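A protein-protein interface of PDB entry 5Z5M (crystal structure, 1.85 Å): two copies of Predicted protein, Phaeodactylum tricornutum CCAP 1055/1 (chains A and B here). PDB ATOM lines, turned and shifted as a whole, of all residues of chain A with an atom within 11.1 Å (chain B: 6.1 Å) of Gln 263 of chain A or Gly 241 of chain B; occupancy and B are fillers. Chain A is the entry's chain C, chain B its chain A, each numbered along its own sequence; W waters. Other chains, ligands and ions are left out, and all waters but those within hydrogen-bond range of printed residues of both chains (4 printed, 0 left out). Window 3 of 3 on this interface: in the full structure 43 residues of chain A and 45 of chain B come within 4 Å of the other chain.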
ATOM      1  N   GLY A 250      27.058  -5.992  14.121  1.00  0.00           N
ATOM      2  CA  GLY A 250      26.555  -5.209  15.236  1.00  0.00           C
ATOM      3  C   GLY A 250      26.300  -6.057  16.465  1.00  0.00           C
ATOM      4  O   GLY A 250      26.722  -5.703  17.563  1.00  0.00           O
ATOM      5  N   PHE A 253      29.787  -7.194  18.039  1.00  0.00           N
ATOM      6  CA  PHE A 253      30.510  -6.190  18.821  1.00  0.00           C
ATOM      7  C   PHE A 253      29.776  -5.903  20.127  1.00  0.00           C
ATOM      8  O   PHE A 253      30.400  -5.689  21.167  1.00  0.00           O
ATOM      9  CB  PHE A 253      30.729  -4.897  18.009  1.00  0.00           C
ATOM     10  CG  PHE A 253      31.701  -5.063  16.869  1.00  0.00           C
ATOM     11  CD1 PHE A 253      32.990  -5.514  17.112  1.00  0.00           C
ATOM     12  CD2 PHE A 253      31.330  -4.777  15.563  1.00  0.00           C
ATOM     13  CE1 PHE A 253      33.888  -5.690  16.076  1.00  0.00           C
ATOM     14  CE2 PHE A 253      32.229  -4.939  14.518  1.00  0.00           C
ATOM     15  CZ  PHE A 253      33.508  -5.401  14.774  1.00  0.00           C
ATOM     16  N   THR A 258      32.219  -3.970  22.930  1.00  0.00           N
ATOM     17  CA  THR A 258      33.088  -3.098  22.143  1.00  0.00           C
ATOM     18  C   THR A 258      32.402  -1.765  21.916  1.00  0.00           C
ATOM     19  O   THR A 258      31.212  -1.726  21.599  1.00  0.00           O
ATOM     20  CB  THR A 258      33.436  -3.727  20.776  1.00  0.00           C
ATOM     21  OG1 THR A 258      34.012  -5.020  20.980  1.00  0.00           O
ATOM     22  CG2 THR A 258      34.420  -2.841  20.000  1.00  0.00           C
ATOM     23  N   PHE A 259      33.136  -0.671  22.081  1.00  0.00           N
ATOM     24  CA  PHE A 259      32.523   0.640  21.916  1.00  0.00           C
ATOM     25  C   PHE A 259      32.081   0.864  20.476  1.00  0.00           C
ATOM     26  O   PHE A 259      32.868   0.704  19.549  1.00  0.00           O
ATOM     27  CB  PHE A 259      33.465   1.766  22.330  1.00  0.00           C
ATOM     28  CG  PHE A 259      32.892   3.132  22.074  1.00  0.00           C
ATOM     29  CD1 PHE A 259      31.970   3.684  22.952  1.00  0.00           C
ATOM     30  CD2 PHE A 259      33.240   3.845  20.937  1.00  0.00           C
ATOM     31  CE1 PHE A 259      31.425   4.931  22.716  1.00  0.00           C
ATOM     32  CE2 PHE A 259      32.699   5.096  20.694  1.00  0.00           C
ATOM     33  CZ  PHE A 259      31.790   5.639  21.585  1.00  0.00           C
ATOM     34  N   THR A 260      30.812   1.221  20.308  1.00  0.00           N
ATOM     35  CA  THR A 260      30.261   1.600  19.011  1.00  0.00           C
ATOM     36  C   THR A 260      29.339   2.802  19.198  1.00  0.00           C
ATOM     37  O   THR A 260      28.866   3.067  20.307  1.00  0.00           O
ATOM     38  CB  THR A 260      29.465   0.452  18.337  1.00  0.00           C
ATOM     39  OG1 THR A 260      28.375   0.060  19.180  1.00  0.00           O
ATOM     40  CG2 THR A 260      30.355  -0.765  18.049  1.00  0.00           C
ATOM     41  N   SER A 261      29.085   3.525  18.115  1.00  0.00           N
ATOM     42  CA  SER A 261      28.168   4.661  18.158  1.00  0.00           C
ATOM     43  C   SER A 261      26.742   4.179  18.405  1.00  0.00           C
ATOM     44  O   SER A 261      26.415   3.031  18.091  1.00  0.00           O
ATOM     45  CB  SER A 261      28.246   5.455  16.855  1.00  0.00           C
ATOM     46  OG  SER A 261      29.495   6.115  16.748  1.00  0.00           O
ATOM     47  N   GLY A 262      25.906   5.049  18.969  1.00  0.00           N
ATOM     48  CA  GLY A 262      24.508   4.726  19.217  1.00  0.00           C
ATOM     49  C   GLY A 262      23.826   4.232  17.954  1.00  0.00           C
ATOM     50  O   GLY A 262      23.149   3.202  17.958  1.00  0.00           O
ATOM     51  N   GLN A 263      23.994   4.988  16.874  1.00  0.00           N
ATOM     52  CA  GLN A 263      23.735   4.485  15.531  1.00  0.00           C
ATOM     53  C   GLN A 263      25.073   3.996  15.004  1.00  0.00           C
ATOM     54  O   GLN A 263      25.892   4.801  14.553  1.00  0.00           O
ATOM     55  CB  GLN A 263      23.154   5.567  14.622  1.00  0.00           C
ATOM     56  CG  GLN A 263      22.957   5.125  13.181  1.00  0.00           C
ATOM     57  CD  GLN A 263      21.677   4.325  12.977  1.00  0.00           C
ATOM     58  OE1 GLN A 263      20.600   4.731  13.411  1.00  0.00           O
ATOM     59  NE2 GLN A 263      21.794   3.186  12.318  1.00  0.00           N
ATOM     60  N   PRO A 264      25.320   2.683  15.087  1.00  0.00           N
ATOM     61  CA  PRO A 264      26.676   2.193  14.816  1.00  0.00           C
ATOM     62  C   PRO A 264      27.116   2.489  13.392  1.00  0.00           C
ATOM     63  O   PRO A 264      26.283   2.475  12.482  1.00  0.00           O
ATOM     64  CB  PRO A 264      26.565   0.684  15.057  1.00  0.00           C
ATOM     65  CG  PRO A 264      25.116   0.376  14.932  1.00  0.00           C
ATOM     66  CD  PRO A 264      24.392   1.592  15.425  1.00  0.00           C
ATOM     67  N   PHE A 265      28.403   2.761  13.205  1.00  0.00           N
ATOM     68  CA  PHE A 265      28.911   2.996  11.867  1.00  0.00           C
ATOM     69  C   PHE A 265      28.689   1.742  11.044  1.00  0.00           C
ATOM     70  O   PHE A 265      28.244   1.825   9.913  1.00  0.00           O
ATOM     71  CB  PHE A 265      30.392   3.376  11.878  1.00  0.00           C
ATOM     72  CG  PHE A 265      30.971   3.555  10.508  1.00  0.00           C
ATOM     73  CD1 PHE A 265      30.536   4.582   9.688  1.00  0.00           C
ATOM     74  CD2 PHE A 265      31.939   2.686  10.031  1.00  0.00           C
ATOM     75  CE1 PHE A 265      31.056   4.740   8.412  1.00  0.00           C
ATOM     76  CE2 PHE A 265      32.466   2.841   8.762  1.00  0.00           C
ATOM     77  CZ  PHE A 265      32.020   3.865   7.950  1.00  0.00           C
ATOM     78  N   LEU A 266      28.979   0.585  11.632  1.00  0.00           N
ATOM     79  CA  LEU A 266      28.726  -0.696  10.978  1.00  0.00           C
ATOM     80  C   LEU A 266      27.858  -1.568  11.868  1.00  0.00           C
ATOM     81  O   LEU A 266      28.168  -1.786  13.044  1.00  0.00           O
ATOM     82  CB  LEU A 266      30.031  -1.424  10.654  1.00  0.00           C
ATOM     83  CG  LEU A 266      31.005  -0.783   9.661  1.00  0.00           C
ATOM     84  CD1 LEU A 266      32.288  -1.611   9.621  1.00  0.00           C
ATOM     85  CD2 LEU A 266      30.399  -0.630   8.257  1.00  0.00           C
ATOM     86  N   ASP A 267      26.768  -2.064  11.301  1.00  0.00           N
ATOM     87  CA  ASP A 267      25.847  -2.925  12.030  1.00  0.00           C
ATOM     88  C   ASP A 267      25.705  -4.241  11.275  1.00  0.00           C
ATOM     89  O   ASP A 267      26.314  -5.252  11.624  1.00  0.00           O
ATOM     90  CB  ASP A 267      24.490  -2.233  12.188  1.00  0.00           C
ATOM     91  CG  ASP A 267      23.502  -3.055  12.989  1.00  0.00           C
ATOM     92  OD1 ASP A 267      23.940  -3.857  13.840  1.00  0.00           O
ATOM     93  OD2 ASP A 267      22.283  -2.889  12.770  1.00  0.00           O
ATOM     94  N   THR A 268      24.905  -4.208  10.221  1.00  0.00           N
ATOM     95  CA  THR A 268      24.762  -5.348   9.332  1.00  0.00           C
ATOM     96  C   THR A 268      25.539  -5.073   8.049  1.00  0.00           C
ATOM     97  O   THR A 268      25.380  -4.019   7.441  1.00  0.00           O
ATOM     98  CB  THR A 268      23.283  -5.619   9.029  1.00  0.00           C
ATOM     99  OG1 THR A 268      22.659  -6.199  10.184  1.00  0.00           O
ATOM    100  CG2 THR A 268      23.152  -6.565   7.873  1.00  0.00           C
ATOM    101  N   PRO A 290      34.725  -2.118  14.289  1.00  0.00           N
ATOM    102  CA  PRO A 290      33.524  -1.274  14.293  1.00  0.00           C
ATOM    103  C   PRO A 290      33.607  -0.109  13.298  1.00  0.00           C
ATOM    104  O   PRO A 290      32.583   0.504  12.997  1.00  0.00           O
ATOM    105  CB  PRO A 290      33.477  -0.731  15.729  1.00  0.00           C
ATOM    106  CG  PRO A 290      34.236  -1.714  16.532  1.00  0.00           C
ATOM    107  CD  PRO A 290      35.314  -2.242  15.634  1.00  0.00           C
ATOM    108  N   TRP A 291      34.807   0.177  12.798  1.00  0.00           N
ATOM    109  CA  TRP A 291      35.050   1.392  12.008  1.00  0.00           C
ATOM    110  C   TRP A 291      35.586   1.155  10.597  1.00  0.00           C
ATOM    111  O   TRP A 291      35.894   2.108   9.871  1.00  0.00           O
ATOM    112  CB  TRP A 291      36.028   2.282  12.758  1.00  0.00           C
ATOM    113  CG  TRP A 291      35.673   2.406  14.194  1.00  0.00           C
ATOM    114  CD1 TRP A 291      36.292   1.801  15.253  1.00  0.00           C
ATOM    115  CD2 TRP A 291      34.596   3.168  14.736  1.00  0.00           C
ATOM    116  NE1 TRP A 291      35.672   2.157  16.423  1.00  0.00           N
ATOM    117  CE2 TRP A 291      34.626   2.996  16.133  1.00  0.00           C
ATOM    118  CE3 TRP A 291      33.615   3.992  14.177  1.00  0.00           C
ATOM    119  CZ2 TRP A 291      33.702   3.608  16.979  1.00  0.00           C
ATOM    120  CZ3 TRP A 291      32.703   4.602  15.016  1.00  0.00           C
ATOM    121  CH2 TRP A 291      32.751   4.407  16.402  1.00  0.00           C
ATOM    122  N   ARG B 132      19.840   1.560  18.897  1.00  0.00           N
ATOM    123  CA  ARG B 132      18.688   2.058  18.158  1.00  0.00           C
ATOM    124  C   ARG B 132      17.921   0.914  17.507  1.00  0.00           C
ATOM    125  O   ARG B 132      18.454   0.219  16.642  1.00  0.00           O
ATOM    126  CB  ARG B 132      19.134   3.067  17.101  1.00  0.00           C
ATOM    127  CG  ARG B 132      19.658   4.353  17.698  1.00  0.00           C
ATOM    128  CD  ARG B 132      19.976   5.373  16.632  1.00  0.00           C
ATOM    129  NE  ARG B 132      20.322   6.660  17.224  1.00  0.00           N
ATOM    130  CZ  ARG B 132      19.442   7.622  17.482  1.00  0.00           C
ATOM    131  NH1 ARG B 132      18.159   7.443  17.201  1.00  0.00           N
ATOM    132  NH2 ARG B 132      19.848   8.763  18.020  1.00  0.00           N
ATOM    133  N   MET B 168      21.280  10.151  22.663  1.00  0.00           N
ATOM    134  CA  MET B 168      20.004   9.869  22.006  1.00  0.00           C
ATOM    135  C   MET B 168      18.894  10.782  22.513  1.00  0.00           C
ATOM    136  O   MET B 168      18.046  11.222  21.744  1.00  0.00           O
ATOM    137  CB  MET B 168      19.603   8.402  22.205  1.00  0.00           C
ATOM    138  CG  MET B 168      20.507   7.421  21.492  1.00  0.00           C
ATOM    139  SD  MET B 168      20.026   5.712  21.808  1.00  0.00           S
ATOM    140  CE  MET B 168      21.358   4.840  20.988  1.00  0.00           C
ATOM    141  N   ARG B 205      18.680   6.213   2.005  1.00  0.00           N
ATOM    142  CA  ARG B 205      18.500   6.169   3.454  1.00  0.00           C
ATOM    143  C   ARG B 205      17.614   4.979   3.801  1.00  0.00           C
ATOM    144  O   ARG B 205      16.519   4.837   3.259  1.00  0.00           O
ATOM    145  CB  ARG B 205      17.882   7.463   3.983  1.00  0.00           C
ATOM    146  CG  ARG B 205      17.829   7.528   5.515  1.00  0.00           C
ATOM    147  CD  ARG B 205      17.149   8.800   6.015  1.00  0.00           C
ATOM    148  NE  ARG B 205      17.937   9.997   5.742  1.00  0.00           N
ATOM    149  CZ  ARG B 205      17.630  10.907   4.822  1.00  0.00           C
ATOM    150  NH1 ARG B 205      16.536  10.775   4.082  1.00  0.00           N
ATOM    151  NH2 ARG B 205      18.413  11.962   4.650  1.00  0.00           N
ATOM    152  N   SER B 207      16.977   3.945   7.192  1.00  0.00           N
ATOM    153  CA  SER B 207      16.273   4.196   8.445  1.00  0.00           C
ATOM    154  C   SER B 207      16.647   5.579   8.980  1.00  0.00           C
ATOM    155  O   SER B 207      17.715   6.104   8.645  1.00  0.00           O
ATOM    156  CB  SER B 207      16.586   3.103   9.475  1.00  0.00           C
ATOM    157  OG  SER B 207      17.878   3.268  10.028  1.00  0.00           O
ATOM    158  N   PRO B 208      15.761   6.197   9.783  1.00  0.00           N
ATOM    159  CA  PRO B 208      14.435   5.717  10.198  1.00  0.00           C
ATOM    160  C   PRO B 208      13.453   5.666   9.027  1.00  0.00           C
ATOM    161  O   PRO B 208      13.553   6.493   8.121  1.00  0.00           O
ATOM    162  CB  PRO B 208      14.001   6.751  11.239  1.00  0.00           C
ATOM    163  CG  PRO B 208      14.717   7.993  10.848  1.00  0.00           C
ATOM    164  CD  PRO B 208      16.049   7.536  10.327  1.00  0.00           C
ATOM    165  N   THR B 239      21.177  13.575   8.181  1.00  0.00           N
ATOM    166  CA  THR B 239      20.483  13.260   9.423  1.00  0.00           C
ATOM    167  C   THR B 239      20.899  11.902   9.983  1.00  0.00           C
ATOM    168  O   THR B 239      21.289  11.011   9.232  1.00  0.00           O
ATOM    169  CB  THR B 239      18.955  13.264   9.221  1.00  0.00           C
ATOM    170  OG1 THR B 239      18.607  12.327   8.191  1.00  0.00           O
ATOM    171  CG2 THR B 239      18.478  14.646   8.813  1.00  0.00           C
ATOM    172  N   VAL B 240      20.816  11.760  11.305  1.00  0.00           N
ATOM    173  CA  VAL B 240      21.112  10.495  11.972  1.00  0.00           C
ATOM    174  C   VAL B 240      20.256   9.370  11.391  1.00  0.00           C
ATOM    175  O   VAL B 240      19.051   9.533  11.191  1.00  0.00           O
ATOM    176  CB  VAL B 240      20.880  10.603  13.499  1.00  0.00           C
ATOM    177  CG1 VAL B 240      20.972   9.231  14.167  1.00  0.00           C
ATOM    178  CG2 VAL B 240      21.878  11.572  14.115  1.00  0.00           C
ATOM    179  N   GLY B 241      20.889   8.238  11.094  1.00  0.00           N
ATOM    180  CA  GLY B 241      20.179   7.091  10.562  1.00  0.00           C
ATOM    181  C   GLY B 241      21.084   6.111   9.843  1.00  0.00           C
ATOM    182  O   GLY B 241      22.308   6.236   9.884  1.00  0.00           O
ATOM    183  N   GLN B 242      20.480   5.124   9.189  1.00  0.00           N
ATOM    184  CA  GLN B 242      21.242   4.141   8.443  1.00  0.00           C
ATOM    185  C   GLN B 242      21.142   4.420   6.950  1.00  0.00           C
ATOM    186  O   GLN B 242      20.064   4.717   6.437  1.00  0.00           O
ATOM    187  CB  GLN B 242      20.748   2.727   8.754  1.00  0.00           C
ATOM    188  CG  GLN B 242      21.618   1.643   8.177  1.00  0.00           C
ATOM    189  CD  GLN B 242      21.110   0.251   8.508  1.00  0.00           C
ATOM    190  OE1 GLN B 242      19.913  -0.029   8.412  1.00  0.00           O
ATOM    191  NE2 GLN B 242      22.021  -0.627   8.914  1.00  0.00           N
ATOM    192  N   TYR B 243      22.272   4.321   6.260  1.00  0.00           N
ATOM    193  CA  TYR B 243      22.338   4.594   4.821  1.00  0.00           C
ATOM    194  C   TYR B 243      22.972   3.441   4.044  1.00  0.00           C
ATOM    195  O   TYR B 243      23.587   2.549   4.630  1.00  0.00           O
ATOM    196  CB  TYR B 243      23.128   5.885   4.564  1.00  0.00           C
ATOM    197  CG  TYR B 243      22.485   7.139   5.123  1.00  0.00           C
ATOM    198  CD1 TYR B 243      22.554   7.434   6.482  1.00  0.00           C
ATOM    199  CD2 TYR B 243      21.825   8.038   4.291  1.00  0.00           C
ATOM    200  CE1 TYR B 243      21.964   8.575   7.001  1.00  0.00           C
ATOM    201  CE2 TYR B 243      21.230   9.188   4.803  1.00  0.00           C
ATOM    202  CZ  TYR B 243      21.309   9.454   6.157  1.00  0.00           C
ATOM    203  OH  TYR B 243      20.726  10.591   6.678  1.00  0.00           O
ATOM    204  N   PHE B 273      25.962   1.713   6.116  1.00  0.00           N
ATOM    205  CA  PHE B 273      26.608   2.421   7.222  1.00  0.00           C
ATOM    206  C   PHE B 273      25.668   3.356   7.990  1.00  0.00           C
ATOM    207  O   PHE B 273      24.624   3.782   7.484  1.00  0.00           O
ATOM    208  CB  PHE B 273      27.812   3.218   6.706  1.00  0.00           C
ATOM    209  CG  PHE B 273      27.439   4.399   5.849  1.00  0.00           C
ATOM    210  CD1 PHE B 273      27.134   4.231   4.509  1.00  0.00           C
ATOM    211  CD2 PHE B 273      27.392   5.673   6.388  1.00  0.00           C
ATOM    212  CE1 PHE B 273      26.796   5.314   3.715  1.00  0.00           C
ATOM    213  CE2 PHE B 273      27.052   6.762   5.601  1.00  0.00           C
ATOM    214  CZ  PHE B 273      26.755   6.584   4.265  1.00  0.00           C
ATOM    215  N   GLY B 274      26.057   3.680   9.220  1.00  0.00           N
ATOM    216  CA  GLY B 274      25.252   4.539  10.064  1.00  0.00           C
ATOM    217  C   GLY B 274      25.900   5.889  10.283  1.00  0.00           C
ATOM    218  O   GLY B 274      27.129   5.990  10.353  1.00  0.00           O
ATOM    219  N   ILE B 275      25.065   6.922  10.375  1.00  0.00           N
ATOM    220  CA  ILE B 275      25.499   8.263  10.753  1.00  0.00           C
ATOM    221  C   ILE B 275      24.951   8.594  12.142  1.00  0.00           C
ATOM    222  O   ILE B 275      23.748   8.532  12.373  1.00  0.00           O
ATOM    223  CB  ILE B 275      25.042   9.321   9.738  1.00  0.00           C
ATOM    224  CG1 ILE B 275      25.796   9.128   8.413  1.00  0.00           C
ATOM    225  CG2 ILE B 275      25.276  10.741  10.292  1.00  0.00           C
ATOM    226  CD1 ILE B 275      25.196   9.890   7.258  1.00  0.00           C
ATOM    227  N   ASP B 276      25.835   8.941  13.067  1.00  0.00           N
ATOM    228  CA  ASP B 276      25.438   9.104  14.463  1.00  0.00           C
ATOM    229  C   ASP B 276      25.421  10.565  14.936  1.00  0.00           C
ATOM    230  O   ASP B 276      24.805  10.876  15.949  1.00  0.00           O
ATOM    231  CB  ASP B 276      26.369   8.290  15.361  1.00  0.00           C
ATOM    232  CG  ASP B 276      25.943   8.312  16.821  1.00  0.00           C
ATOM    233  OD1 ASP B 276      24.840   7.809  17.133  1.00  0.00           O
ATOM    234  OD2 ASP B 276      26.706   8.843  17.658  1.00  0.00           O
ATOM    235  N   TYR B 282      31.402  13.233   7.782  1.00  0.00           N
ATOM    236  CA  TYR B 282      31.609  11.809   7.545  1.00  0.00           C
ATOM    237  C   TYR B 282      32.182  11.624   6.154  1.00  0.00           C
ATOM    238  O   TYR B 282      31.595  12.063   5.172  1.00  0.00           O
ATOM    239  CB  TYR B 282      30.305  11.022   7.684  1.00  0.00           C
ATOM    240  CG  TYR B 282      29.908  10.658   9.097  1.00  0.00           C
ATOM    241  CD1 TYR B 282      29.651  11.637  10.048  1.00  0.00           C
ATOM    242  CD2 TYR B 282      29.759   9.331   9.471  1.00  0.00           C
ATOM    243  CE1 TYR B 282      29.272  11.297  11.337  1.00  0.00           C
ATOM    244  CE2 TYR B 282      29.380   8.983  10.750  1.00  0.00           C
ATOM    245  CZ  TYR B 282      29.143   9.968  11.681  1.00  0.00           C
ATOM    246  OH  TYR B 282      28.763   9.625  12.957  1.00  0.00           O
HETATM  247  O   HOH W   1      26.724   7.595  20.122  1.00  0.00           O
HETATM  248  O   HOH W   2      27.981   6.077  13.059  1.00  0.00           O
HETATM  249  O   HOH W   3      17.807   4.824  12.725  1.00  0.00           O
HETATM  250  O   HOH W   4      29.913   6.979  14.265  1.00  0.00           O
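OD1 of Asp 276 of chain B sits at hydrogen-bond distance from N of Gly 262 of chain A (3.5 Å). The backbone NH of Gly 274 of chain B is in hydrogen-bond range of the backbone carbonyl oxygen of Phe 265 of chain A (3.0 Å). OD1 of Asp 276 of chain B lies within hydrogen-bond range of N of Gln 263 of chain A (3.0 Å). The backbone NH (N) of Gly 274 of chain B lies close to the backbone carbonyl oxygen (O) of Pro 264 of chain A (3.5 Å).
The backbone NH (N) of Tyr 243 of chain B sits at hydrogen-bond distance from the backbone carbonyl oxygen (O) of Phe 273 of chain B (2.7 Å). N of Gln 242 of chain B sits at hydrogen-bond distance from O of Ser 207 of chain B (3.0 Å). The backbone NH of Ile 275 of chain B lies within hydrogen-bond range of the backbone carbonyl oxygen of Gly 241 of chain B, at 2.9 Å. OH of Tyr 282 of chain B is in hydrogen-bond range of N of Asp 276 of chain B, 3.0 Å away.
Among the printed residues, merely in contact across the chains: Phe 265 of chain A with Phe 273 of chain B (3.2 Å), Gln 263 of chain A with Arg 132 of chain B (3.3 Å), Gln 263 of chain A with Gly 241 of chain B (3.5 Å), Gln 263 of chain A with Ile 275 of chain B (3.6 Å), Gly 262 of chain A with Met 168 of chain B (3.6 Å), Ser 261 of chain A with Asp 276 of chain B (3.7 Å), Gly 262 of chain A with Arg 132 of chain B (3.7 Å), Gln 263 of chain A with Gln 242 of chain B (3.7 Å) and Gln 263 of chain A with Gly 274 of chain B (3.9 Å).
Of chain B, only Arg 132 (3.3 Å), Gly 241 (3.5 Å), Gln 242 (3.7 Å), Gly 274 (3.9 Å), Ile 275 (3.6 Å) and Asp 276 (3.0 Å) come within 4 Å of Gln 263 of chain A. Gly 241 of chain B touches just one residue of chain A: Gln 263. Arg 132 of chain B touches just these residues of chain A: Gly 262 (3.7 Å) and Gln 263 (3.3 Å). No residue of chain A comes within 4 Å of Val 240 of chain B. Of the printed residues of chain A, Gln 242 of chain B touches Gln 263. Gly 274 of chain B touches just these residues of chain A: Gln 263 (3.9 Å), Pro 264 (3.3 Å) and Phe 265 (3.0 Å). Of the printed residues of chain B, Pro 264 of chain A touches Gly 274 (3.3 Å). Of the printed residues of chain A, Phe 273 of chain B touches Phe 265. Printed residues of chain B within 4 Å of Phe 265 of chain A: Phe 273 and Gly 274. Printed residues of chain A within 4 Å of Met 168 of chain B: Gly 262. Thr 268 of chain A touches none of the printed residues of chain B. The nearest residue of chain B that does not touch Gln 263 of chain A is Val 240 of chain B (4.3 Å). The nearest printed residue of chain B that does not touch Pro 264 of chain A is Phe 273 of chain B (4.6 Å).
Hydrophobic or aromatic side chains of chain B that line the printed part of chain A: Met 168 and Phe 273. Among the printed residues, no Asp or Glu carboxylate lies within 4 Å of a Lys or Arg side-chain nitrogen of the other chain.
No position is printed for both chains. Of the 13 pairs that touch across the chains among the printed residues, none has its exchanged pair printed and touching as well.
Water W4 bridges OG of Ser 261 of chain A (2.7 Å) and OH of Tyr 282 of chain B (3.2 Å). Water W1 lies within hydrogen-bond range of the side-chain carboxylate (OD2) of Asp 276 of chain B (2.8 Å) and the backbone NH (N) of Gly 262 of chain A (2.9 Å). Water W2 lies within hydrogen-bond range of the backbone carbonyl oxygen of Gly 274 of chain B (2.8 Å), the backbone carbonyl oxygen of Gln 263 of chain A (2.9 Å) and the backbone NH of Phe 265 of chain A (3.3 Å). Water W3 bridges the side-chain amide oxygen of Gln 263 of chain A (2.9 Å) and the side-chain hydroxyl of Ser 207 of chain B (3.1 Å).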
